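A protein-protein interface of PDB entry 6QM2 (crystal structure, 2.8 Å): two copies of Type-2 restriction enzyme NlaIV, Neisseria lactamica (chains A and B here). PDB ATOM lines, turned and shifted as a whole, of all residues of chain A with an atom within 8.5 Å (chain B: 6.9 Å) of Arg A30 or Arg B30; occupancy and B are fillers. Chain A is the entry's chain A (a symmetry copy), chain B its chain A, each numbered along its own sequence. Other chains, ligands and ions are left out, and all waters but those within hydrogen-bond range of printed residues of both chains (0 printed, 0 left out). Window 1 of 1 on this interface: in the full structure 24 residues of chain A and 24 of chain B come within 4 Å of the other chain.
Among the printed residues, merely in contact across the chains: Gly A27 with Phe B32 (3.1 Å), Gln A28 with Arg B30 (3.9 Å), Gln A28 with Phe B31 (3.8 Å), Ile A29 with Ile B29 (3.8 Å), Ile A29 with Arg B30 (3.6 Å), Ile A29 with Phe B31 (3.7 Å), Arg A30 with Gln B28 (3.9 Å), Arg A30 with Ile B29 (3.6 Å), Phe A31 with Gln B28 (3.8 Å), Phe A31 with Ile B29 (3.7 Å), Phe A32 with Phe B32 (3.9 Å), Ile A49 with Phe B31 (3.7 Å), Ile A49 with Ile B38 (3.9 Å), Ile A49 with Val B40 (3.4 Å), Trp A53 with Phe B31 (3.9 Å) and Trp A53 with Ile B38 (3.2 Å).
The guanidinium group of Arg B30 sits at hydrogen-bond distance from the side-chain amide oxygen of Gln B28, at 3.1 Å. O of Gly A27 lies within hydrogen-bond range of ND2 of Asn A137, 3.2 Å away. The guanidinium group (NH2) of Arg A30 is in hydrogen-bond range of the side-chain amide oxygen (OE1) of Gln A28. N of Val B40 lies within hydrogen-bond range of O of Ile B29, 3.1 Å away. The guanidinium group (NE) of Arg A30 is in salt-bridge range of the side-chain carboxylate (OD1) of Asp A37, 2.7 Å away. The backbone carbonyl oxygen (O) of Ile B38 lies within hydrogen-bond range of the backbone NH (N) of Phe B31 (3.1 Å).
Gln A28 touches Arg B30, and with the chains exchanged Arg A30 touches Gln B28. Gln A28 touches Phe B32, and with the chains exchanged Phe A32 touches Gln B28. Ile A29 touches its own counterpart, Ile B29. Arg A30 touches its own counterpart, Arg B30. Positions printed for both chains: 28, 29, 30, 31, 32, 37, 38, 39, 40 and 135. Of the 19 pairs that touch across the chains among the printed residues, 13 have their exchanged pair printed and touching as well.
The backbone carbonyl oxygen (O) of Phe A32 is in hydrogen-bond range of the backbone NH (N) of Gln B28 (2.8 Å). O of Phe B32 lies within hydrogen-bond range of N of Gln A28, 2.8 Å away. The backbone carbonyl oxygen of Arg B30 is in hydrogen-bond range of the backbone NH of Arg A30 (2.8 Å).
Printed residues of chain A that touch a printed residue of chain B: Gly A27, Gln A28, Ile A29, Arg A30, Phe A31, Phe A32, Ile A49 and Trp A53. Hydrophobic or aromatic side chains of chain A that line the printed part of chain B: Ile A29, Phe A31, Phe A32, Ile A49 and Trp A53. Among the printed residues, 19 pairs touch across the chains. Among the printed residues, no Asp or Glu carboxylate lies within 4 Å of a Lys or Arg side-chain nitrogen of the other chain.
Of chain B, only Gln B28, Ile B29 and Arg B30 come within 4 Å of Arg A30. Of chain A, only Gln A28 (3.9 Å), Ile A29 (3.6 Å) and Arg A30 (2.8 Å) come within 4 Å of Arg B30. Of the printed residues of chain A, Val B40 touches Ile A49. Of the printed residues of chain B, Gly A27 touches Phe B32 (3.1 Å). Val A40 touches none of the printed residues of chain B. The nearest residue of chain B that does not touch Arg A30 is Phe B32 (4.2 Å). The nearest residue of chain A that does not touch Arg B30 is Phe A32 (4.2 Å).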
ATOM      1  N   GLY A  27      22.429   3.586   0.652  1.00  0.00           N
ATOM      2  CA  GLY A  27      21.052   4.073   0.774  1.00  0.00           C
ATOM      3  C   GLY A  27      20.976   5.585   0.702  1.00  0.00           C
ATOM      4  O   GLY A  27      22.004   6.257   0.733  1.00  0.00           O
ATOM      5  N   GLN A  28      19.760   6.120   0.610  1.00  0.00           N
ATOM      6  CA  GLN A  28      19.557   7.566   0.462  1.00  0.00           C
ATOM      7  C   GLN A  28      18.089   7.980   0.605  1.00  0.00           C
ATOM      8  O   GLN A  28      17.188   7.238   0.214  1.00  0.00           O
ATOM      9  CB  GLN A  28      20.086   8.037  -0.897  1.00  0.00           C
ATOM     10  CG  GLN A  28      19.669   7.161  -2.073  1.00  0.00           C
ATOM     11  CD  GLN A  28      20.118   7.726  -3.405  1.00  0.00           C
ATOM     12  OE1 GLN A  28      19.310   7.897  -4.318  1.00  0.00           O
ATOM     13  NE2 GLN A  28      21.412   8.024  -3.523  1.00  0.00           N
ATOM     14  N   ILE A  29      17.865   9.176   1.150  1.00  0.00           N
ATOM     15  CA  ILE A  29      16.520   9.759   1.232  1.00  0.00           C
ATOM     16  C   ILE A  29      16.253  10.410  -0.119  1.00  0.00           C
ATOM     17  O   ILE A  29      17.163  10.992  -0.717  1.00  0.00           O
ATOM     18  CB  ILE A  29      16.381  10.820   2.351  1.00  0.00           C
ATOM     19  CG1 ILE A  29      16.865  10.280   3.706  1.00  0.00           C
ATOM     20  CG2 ILE A  29      14.926  11.277   2.477  1.00  0.00           C
ATOM     21  CD1 ILE A  29      17.085  11.353   4.751  1.00  0.00           C
ATOM     22  N   ARG A  30      15.013  10.317  -0.593  1.00  0.00           N
ATOM     23  CA  ARG A  30      14.666  10.807  -1.924  1.00  0.00           C
ATOM     24  C   ARG A  30      13.213  11.281  -1.986  1.00  0.00           C
ATOM     25  O   ARG A  30      12.312  10.583  -1.519  1.00  0.00           O
ATOM     26  CB  ARG A  30      14.942   9.707  -2.968  1.00  0.00           C
ATOM     27  CG  ARG A  30      15.466  10.242  -4.292  1.00  0.00           C
ATOM     28  CD  ARG A  30      16.200   9.206  -5.125  1.00  0.00           C
ATOM     29  NE  ARG A  30      16.793   9.827  -6.316  1.00  0.00           N
ATOM     30  CZ  ARG A  30      17.911  10.566  -6.347  1.00  0.00           C
ATOM     31  NH1 ARG A  30      18.328  11.075  -7.507  1.00  0.00           N
ATOM     32  NH2 ARG A  30      18.623  10.809  -5.245  1.00  0.00           N
ATOM     33  N   PHE A  31      12.997  12.469  -2.555  1.00  0.00           N
ATOM     34  CA  PHE A  31      11.661  13.059  -2.678  1.00  0.00           C
ATOM     35  C   PHE A  31      11.201  13.025  -4.128  1.00  0.00           C
ATOM     36  O   PHE A  31      11.857  13.588  -4.999  1.00  0.00           O
ATOM     37  CB  PHE A  31      11.654  14.504  -2.167  1.00  0.00           C
ATOM     38  CG  PHE A  31      10.338  15.213  -2.370  1.00  0.00           C
ATOM     39  CD1 PHE A  31       9.170  14.705  -1.817  1.00  0.00           C
ATOM     40  CD2 PHE A  31      10.266  16.385  -3.120  1.00  0.00           C
ATOM     41  CE1 PHE A  31       7.954  15.352  -2.001  1.00  0.00           C
ATOM     42  CE2 PHE A  31       9.054  17.037  -3.305  1.00  0.00           C
ATOM     43  CZ  PHE A  31       7.895  16.520  -2.747  1.00  0.00           C
ATOM     44  N   PHE A  32      10.067  12.368  -4.366  1.00  0.00           N
ATOM     45  CA  PHE A  32       9.454  12.265  -5.684  1.00  0.00           C
ATOM     46  C   PHE A  32       8.254  13.199  -5.708  1.00  0.00           C
ATOM     47  O   PHE A  32       7.525  13.294  -4.725  1.00  0.00           O
ATOM     48  CB  PHE A  32       8.985  10.825  -5.949  1.00  0.00           C
ATOM     49  CG  PHE A  32      10.093   9.797  -5.911  1.00  0.00           C
ATOM     50  CD1 PHE A  32      10.568   9.300  -4.694  1.00  0.00           C
ATOM     51  CD2 PHE A  32      10.653   9.307  -7.091  1.00  0.00           C
ATOM     52  CE1 PHE A  32      11.586   8.353  -4.658  1.00  0.00           C
ATOM     53  CE2 PHE A  32      11.674   8.361  -7.059  1.00  0.00           C
ATOM     54  CZ  PHE A  32      12.141   7.882  -5.843  1.00  0.00           C
ATOM     55  N   LEU A  33       8.068  13.903  -6.819  1.00  0.00           N
ATOM     56  CA  LEU A  33       6.842  14.666  -7.076  1.00  0.00           C
ATOM     57  C   LEU A  33       6.730  14.858  -8.585  1.00  0.00           C
ATOM     58  O   LEU A  33       7.707  15.245  -9.231  1.00  0.00           O
ATOM     59  CB  LEU A  33       6.859  16.017  -6.342  1.00  0.00           C
ATOM     60  CG  LEU A  33       5.729  17.026  -6.612  1.00  0.00           C
ATOM     61  CD1 LEU A  33       4.372  16.465  -6.215  1.00  0.00           C
ATOM     62  CD2 LEU A  33       5.990  18.336  -5.885  1.00  0.00           C
ATOM     63  N   VAL A  36       9.800  14.412 -11.369  1.00  0.00           N
ATOM     64  CA  VAL A  36      11.140  14.773 -10.910  1.00  0.00           C
ATOM     65  C   VAL A  36      11.369  14.186  -9.522  1.00  0.00           C
ATOM     66  O   VAL A  36      10.488  14.251  -8.657  1.00  0.00           O
ATOM     67  CB  VAL A  36      11.336  16.305 -10.877  1.00  0.00           C
ATOM     68  CG1 VAL A  36      12.747  16.663 -10.409  1.00  0.00           C
ATOM     69  CG2 VAL A  36      11.041  16.907 -12.243  1.00  0.00           C
ATOM     70  N   ASP A  37      12.545  13.596  -9.327  1.00  0.00           N
ATOM     71  CA  ASP A  37      12.972  13.116  -8.021  1.00  0.00           C
ATOM     72  C   ASP A  37      14.340  13.709  -7.690  1.00  0.00           C
ATOM     73  O   ASP A  37      15.171  13.891  -8.583  1.00  0.00           O
ATOM     74  CB  ASP A  37      12.965  11.578  -7.969  1.00  0.00           C
ATOM     75  CG  ASP A  37      14.051  10.938  -8.819  1.00  0.00           C
ATOM     76  OD1 ASP A  37      15.192  10.798  -8.328  1.00  0.00           O
ATOM     77  OD2 ASP A  37      13.750  10.542  -9.966  1.00  0.00           O
ATOM     78  N   ILE A  38      14.557  14.024  -6.415  1.00  0.00           N
ATOM     79  CA  ILE A  38      15.807  14.637  -5.961  1.00  0.00           C
ATOM     80  C   ILE A  38      16.342  13.942  -4.722  1.00  0.00           C
ATOM     81  O   ILE A  38      15.574  13.394  -3.932  1.00  0.00           O
ATOM     82  CB  ILE A  38      15.627  16.141  -5.639  1.00  0.00           C
ATOM     83  CG1 ILE A  38      14.716  16.346  -4.411  1.00  0.00           C
ATOM     84  CG2 ILE A  38      15.065  16.874  -6.850  1.00  0.00           C
ATOM     85  CD1 ILE A  38      14.580  17.779  -3.953  1.00  0.00           C
ATOM     86  N   ILE A  39      17.659  13.995  -4.552  1.00  0.00           N
ATOM     87  CA  ILE A  39      18.303  13.599  -3.302  1.00  0.00           C
ATOM     88  C   ILE A  39      17.851  14.562  -2.198  1.00  0.00           C
ATOM     89  O   ILE A  39      17.606  15.742  -2.461  1.00  0.00           O
ATOM     90  CB  ILE A  39      19.854  13.593  -3.440  1.00  0.00           C
ATOM     91  CG1 ILE A  39      20.510  12.779  -2.316  1.00  0.00           C
ATOM     92  CG2 ILE A  39      20.431  15.009  -3.496  1.00  0.00           C
ATOM     93  CD1 ILE A  39      20.506  11.287  -2.559  1.00  0.00           C
ATOM     94  N   VAL A  40      17.717  14.047  -0.979  1.00  0.00           N
ATOM     95  CA  VAL A  40      17.433  14.868   0.195  1.00  0.00           C
ATOM     96  C   VAL A  40      18.620  14.739   1.147  1.00  0.00           C
ATOM     97  O   VAL A  40      18.994  13.628   1.529  1.00  0.00           O
ATOM     98  CB  VAL A  40      16.120  14.434   0.872  1.00  0.00           C
ATOM     99  CG1 VAL A  40      15.886  15.210   2.168  1.00  0.00           C
ATOM    100  CG2 VAL A  40      14.954  14.597  -0.098  1.00  0.00           C
ATOM    101  N   LYS A  41      19.202  15.878   1.521  1.00  0.00           N
ATOM    102  CA  LYS A  41      20.456  15.910   2.278  1.00  0.00           C
ATOM    103  C   LYS A  41      20.313  16.460   3.705  1.00  0.00           C
ATOM    104  O   LYS A  41      21.313  16.862   4.303  1.00  0.00           O
ATOM    105  CB  LYS A  41      21.498  16.735   1.512  1.00  0.00           C
ATOM    106  CG  LYS A  41      21.711  16.314   0.066  1.00  0.00           C
ATOM    107  CD  LYS A  41      22.815  17.134  -0.585  1.00  0.00           C
ATOM    108  CE  LYS A  41      22.772  17.031  -2.100  1.00  0.00           C
ATOM    109  NZ  LYS A  41      23.770  17.925  -2.745  1.00  0.00           N
ATOM    110  N   ILE A  49      14.662   8.128  11.031  1.00  0.00           N
ATOM    111  CA  ILE A  49      14.098   7.274   9.990  1.00  0.00           C
ATOM    112  C   ILE A  49      14.695   5.860   9.937  1.00  0.00           C
ATOM    113  O   ILE A  49      14.075   4.973   9.353  1.00  0.00           O
ATOM    114  CB  ILE A  49      14.160   7.989   8.604  1.00  0.00           C
ATOM    115  CG1 ILE A  49      12.884   7.723   7.802  1.00  0.00           C
ATOM    116  CG2 ILE A  49      15.398   7.616   7.793  1.00  0.00           C
ATOM    117  CD1 ILE A  49      11.675   8.492   8.302  1.00  0.00           C
ATOM    118  N   TRP A  53      12.741   2.400   9.168  1.00  0.00           N
ATOM    119  CA  TRP A  53      13.263   1.490   8.146  1.00  0.00           C
ATOM    120  C   TRP A  53      13.386   0.054   8.636  1.00  0.00           C
ATOM    121  O   TRP A  53      13.053  -0.876   7.900  1.00  0.00           O
ATOM    122  CB  TRP A  53      14.626   1.979   7.639  1.00  0.00           C
ATOM    123  CG  TRP A  53      15.292   1.047   6.677  1.00  0.00           C
ATOM    124  CD1 TRP A  53      15.149   1.030   5.322  1.00  0.00           C
ATOM    125  CD2 TRP A  53      16.205  -0.005   6.999  1.00  0.00           C
ATOM    126  NE1 TRP A  53      15.918   0.033   4.778  1.00  0.00           N
ATOM    127  CE2 TRP A  53      16.577  -0.620   5.785  1.00  0.00           C
ATOM    128  CE3 TRP A  53      16.741  -0.492   8.197  1.00  0.00           C
ATOM    129  CZ2 TRP A  53      17.471  -1.696   5.732  1.00  0.00           C
ATOM    130  CZ3 TRP A  53      17.635  -1.564   8.144  1.00  0.00           C
ATOM    131  CH2 TRP A  53      17.988  -2.154   6.918  1.00  0.00           C
ATOM    132  N   LYS A  60       8.706  -6.575   5.881  1.00  0.00           N
ATOM    133  CA  LYS A  60       8.955  -7.188   4.569  1.00  0.00           C
ATOM    134  C   LYS A  60       9.530  -8.604   4.659  1.00  0.00           C
ATOM    135  O   LYS A  60       9.354  -9.392   3.732  1.00  0.00           O
ATOM    136  CB  LYS A  60       9.880  -6.311   3.717  1.00  0.00           C
ATOM    137  CG  LYS A  60       9.878  -6.674   2.236  1.00  0.00           C
ATOM    138  CD  LYS A  60      10.600  -5.639   1.389  1.00  0.00           C
ATOM    139  CE  LYS A  60      10.283  -5.805  -0.090  1.00  0.00           C
ATOM    140  NZ  LYS A  60      10.724  -4.621  -0.877  1.00  0.00           N
ATOM    141  N   ASN A 135      27.255  14.115  -1.267  1.00  0.00           N
ATOM    142  CA  ASN A 135      26.290  13.742  -2.317  1.00  0.00           C
ATOM    143  C   ASN A 135      24.954  13.198  -1.789  1.00  0.00           C
ATOM    144  O   ASN A 135      24.004  13.061  -2.561  1.00  0.00           O
ATOM    145  CB  ASN A 135      26.907  12.718  -3.285  1.00  0.00           C
ATOM    146  CG  ASN A 135      27.929  13.338  -4.221  1.00  0.00           C
ATOM    147  OD1 ASN A 135      27.624  14.280  -4.956  1.00  0.00           O
ATOM    148  ND2 ASN A 135      29.147  12.805  -4.212  1.00  0.00           N
ATOM    149  N   GLY A 136      24.887  12.875  -0.497  1.00  0.00           N
ATOM    150  CA  GLY A 136      23.655  12.398   0.143  1.00  0.00           C
ATOM    151  C   GLY A 136      23.484  10.888   0.282  1.00  0.00           C
ATOM    152  O   GLY A 136      22.404  10.431   0.672  1.00  0.00           O
ATOM    153  N   ASN A 137      24.529  10.119  -0.033  1.00  0.00           N
ATOM    154  CA  ASN A 137      24.486   8.662   0.088  1.00  0.00           C
ATOM    155  C   ASN A 137      24.728   8.247   1.540  1.00  0.00           C
ATOM    156  O   ASN A 137      25.796   8.509   2.099  1.00  0.00           O
ATOM    157  CB  ASN A 137      25.527   8.008  -0.824  1.00  0.00           C
ATOM    158  CG  ASN A 137      25.204   6.553  -1.126  1.00  0.00           C
ATOM    159  OD1 ASN A 137      25.975   5.652  -0.793  1.00  0.00           O
ATOM    160  ND2 ASN A 137      24.054   6.319  -1.751  1.00  0.00           N
ATOM    161  N   VAL A 138      23.724   7.608   2.140  1.00  0.00           N
ATOM    162  CA  VAL A 138      23.789   7.127   3.525  1.00  0.00           C
ATOM    163  C   VAL A 138      24.418   5.737   3.559  1.00  0.00           C
ATOM    164  O   VAL A 138      24.075   4.879   2.742  1.00  0.00           O
ATOM    165  CB  VAL A 138      22.382   7.042   4.169  1.00  0.00           C
ATOM    166  CG1 VAL A 138      22.476   6.575   5.621  1.00  0.00           C
ATOM    167  CG2 VAL A 138      21.656   8.384   4.078  1.00  0.00           C
ATOM    168  N   GLN B  28       5.921  11.842  -2.895  1.00  0.00           N
ATOM    169  CA  GLN B  28       6.195  11.293  -1.561  1.00  0.00           C
ATOM    170  C   GLN B  28       7.691  11.233  -1.236  1.00  0.00           C
ATOM    171  O   GLN B  28       8.516  11.009  -2.123  1.00  0.00           O
ATOM    172  CB  GLN B  28       5.593   9.889  -1.436  1.00  0.00           C
ATOM    173  CG  GLN B  28       5.869   8.976  -2.625  1.00  0.00           C
ATOM    174  CD  GLN B  28       5.353   7.568  -2.407  1.00  0.00           C
ATOM    175  OE1 GLN B  28       6.099   6.598  -2.549  1.00  0.00           O
ATOM    176  NE2 GLN B  28       4.073   7.448  -2.055  1.00  0.00           N
ATOM    177  N   ILE B  29       8.024  11.416   0.042  1.00  0.00           N
ATOM    178  CA  ILE B  29       9.403  11.259   0.521  1.00  0.00           C
ATOM    179  C   ILE B  29       9.602   9.768   0.762  1.00  0.00           C
ATOM    180  O   ILE B  29       8.685   9.087   1.230  1.00  0.00           O
ATOM    181  CB  ILE B  29       9.686  12.035   1.832  1.00  0.00           C
ATOM    182  CG1 ILE B  29       9.276  13.510   1.713  1.00  0.00           C
ATOM    183  CG2 ILE B  29      11.170  11.948   2.194  1.00  0.00           C
ATOM    184  CD1 ILE B  29       9.197  14.234   3.042  1.00  0.00           C
ATOM    185  N   ARG B  30      10.796   9.267   0.453  1.00  0.00           N
ATOM    186  CA  ARG B  30      11.068   7.835   0.538  1.00  0.00           C
ATOM    187  C   ARG B  30      12.539   7.563   0.867  1.00  0.00           C
ATOM    188  O   ARG B  30      13.430   8.151   0.254  1.00  0.00           O
ATOM    189  CB  ARG B  30      10.652   7.150  -0.777  1.00  0.00           C
ATOM    190  CG  ARG B  30      10.062   5.763  -0.580  1.00  0.00           C
ATOM    191  CD  ARG B  30       9.208   5.288  -1.744  1.00  0.00           C
ATOM    192  NE  ARG B  30       8.564   4.008  -1.425  1.00  0.00           N
ATOM    193  CZ  ARG B  30       7.491   3.840  -0.638  1.00  0.00           C
ATOM    194  NH1 ARG B  30       7.018   2.611  -0.430  1.00  0.00           N
ATOM    195  NH2 ARG B  30       6.879   4.872  -0.055  1.00  0.00           N
ATOM    196  N   PHE B  31      12.778   6.679   1.838  1.00  0.00           N
ATOM    197  CA  PHE B  31      14.132   6.324   2.271  1.00  0.00           C
ATOM    198  C   PHE B  31      14.479   4.914   1.812  1.00  0.00           C
ATOM    199  O   PHE B  31      13.792   3.961   2.169  1.00  0.00           O
ATOM    200  CB  PHE B  31      14.261   6.418   3.795  1.00  0.00           C
ATOM    201  CG  PHE B  31      15.595   5.954   4.322  1.00  0.00           C
ATOM    202  CD1 PHE B  31      16.772   6.558   3.895  1.00  0.00           C
ATOM    203  CD2 PHE B  31      15.678   4.909   5.239  1.00  0.00           C
ATOM    204  CE1 PHE B  31      18.005   6.134   4.374  1.00  0.00           C
ATOM    205  CE2 PHE B  31      16.907   4.483   5.724  1.00  0.00           C
ATOM    206  CZ  PHE B  31      18.074   5.095   5.290  1.00  0.00           C
ATOM    207  N   PHE B  32      15.552   4.801   1.032  1.00  0.00           N
ATOM    208  CA  PHE B  32      16.057   3.528   0.532  1.00  0.00           C
ATOM    209  C   PHE B  32      17.304   3.181   1.332  1.00  0.00           C
ATOM    210  O   PHE B  32      18.108   4.058   1.632  1.00  0.00           O
ATOM    211  CB  PHE B  32      16.422   3.641  -0.957  1.00  0.00           C
ATOM    212  CG  PHE B  32      15.263   4.023  -1.850  1.00  0.00           C
ATOM    213  CD1 PHE B  32      14.854   5.353  -1.964  1.00  0.00           C
ATOM    214  CD2 PHE B  32      14.588   3.055  -2.595  1.00  0.00           C
ATOM    215  CE1 PHE B  32      13.788   5.705  -2.787  1.00  0.00           C
ATOM    216  CE2 PHE B  32      13.520   3.403  -3.419  1.00  0.00           C
ATOM    217  CZ  PHE B  32      13.120   4.729  -3.515  1.00  0.00           C
ATOM    218  N   ASP B  37      12.780  -0.157   1.063  1.00  0.00           N
ATOM    219  CA  ASP B  37      12.427   1.253   0.986  1.00  0.00           C
ATOM    220  C   ASP B  37      11.124   1.487   1.747  1.00  0.00           C
ATOM    221  O   ASP B  37      10.239   0.627   1.746  1.00  0.00           O
ATOM    222  CB  ASP B  37      12.349   1.724  -0.477  1.00  0.00           C
ATOM    223  CG  ASP B  37      11.168   1.145  -1.238  1.00  0.00           C
ATOM    224  OD1 ASP B  37      10.061   1.719  -1.154  1.00  0.00           O
ATOM    225  OD2 ASP B  37      11.359   0.134  -1.949  1.00  0.00           O
ATOM    226  N   ILE B  38      11.022   2.637   2.409  1.00  0.00           N
ATOM    227  CA  ILE B  38       9.847   2.977   3.216  1.00  0.00           C
ATOM    228  C   ILE B  38       9.368   4.387   2.922  1.00  0.00           C
ATOM    229  O   ILE B  38      10.161   5.252   2.550  1.00  0.00           O
ATOM    230  CB  ILE B  38      10.137   2.864   4.733  1.00  0.00           C
ATOM    231  CG1 ILE B  38      11.148   3.934   5.191  1.00  0.00           C
ATOM    232  CG2 ILE B  38      10.647   1.468   5.067  1.00  0.00           C
ATOM    233  CD1 ILE B  38      11.400   3.974   6.680  1.00  0.00           C
ATOM    234  N   ILE B  39       8.072   4.611   3.118  1.00  0.00           N
ATOM    235  CA  ILE B  39       7.504   5.956   3.122  1.00  0.00           C
ATOM    236  C   ILE B  39       8.093   6.727   4.311  1.00  0.00           C
ATOM    237  O   ILE B  39       8.384   6.137   5.354  1.00  0.00           O
ATOM    238  CB  ILE B  39       5.949   5.915   3.197  1.00  0.00           C
ATOM    239  CG1 ILE B  39       5.335   7.254   2.767  1.00  0.00           C
ATOM    240  CG2 ILE B  39       5.451   5.506   4.585  1.00  0.00           C
ATOM    241  CD1 ILE B  39       5.236   7.429   1.269  1.00  0.00           C
ATOM    242  N   VAL B  40       8.289   8.030   4.134  1.00  0.00           N
ATOM    243  CA  VAL B  40       8.706   8.917   5.217  1.00  0.00           C
ATOM    244  C   VAL B  40       7.590   9.934   5.438  1.00  0.00           C
ATOM    245  O   VAL B  40       7.182  10.626   4.503  1.00  0.00           O
ATOM    246  CB  VAL B  40      10.040   9.611   4.884  1.00  0.00           C
ATOM    247  CG1 VAL B  40      10.415  10.629   5.959  1.00  0.00           C
ATOM    248  CG2 VAL B  40      11.137   8.568   4.690  1.00  0.00           C
ATOM    249  N   ASN B 135      -1.224   8.281   4.842  1.00  0.00           N
ATOM    250  CA  ASN B 135      -0.364   7.320   4.129  1.00  0.00           C
ATOM    251  C   ASN B 135       0.975   7.899   3.648  1.00  0.00           C
ATOM    252  O   ASN B 135       1.853   7.141   3.237  1.00  0.00           O
ATOM    253  CB  ASN B 135      -1.111   6.706   2.931  1.00  0.00           C
ATOM    254  CG  ASN B 135      -2.163   5.695   3.353  1.00  0.00           C
ATOM    255  OD1 ASN B 135      -1.861   4.715   4.036  1.00  0.00           O
ATOM    256  ND2 ASN B 135      -3.406   5.920   2.936  1.00  0.00           N
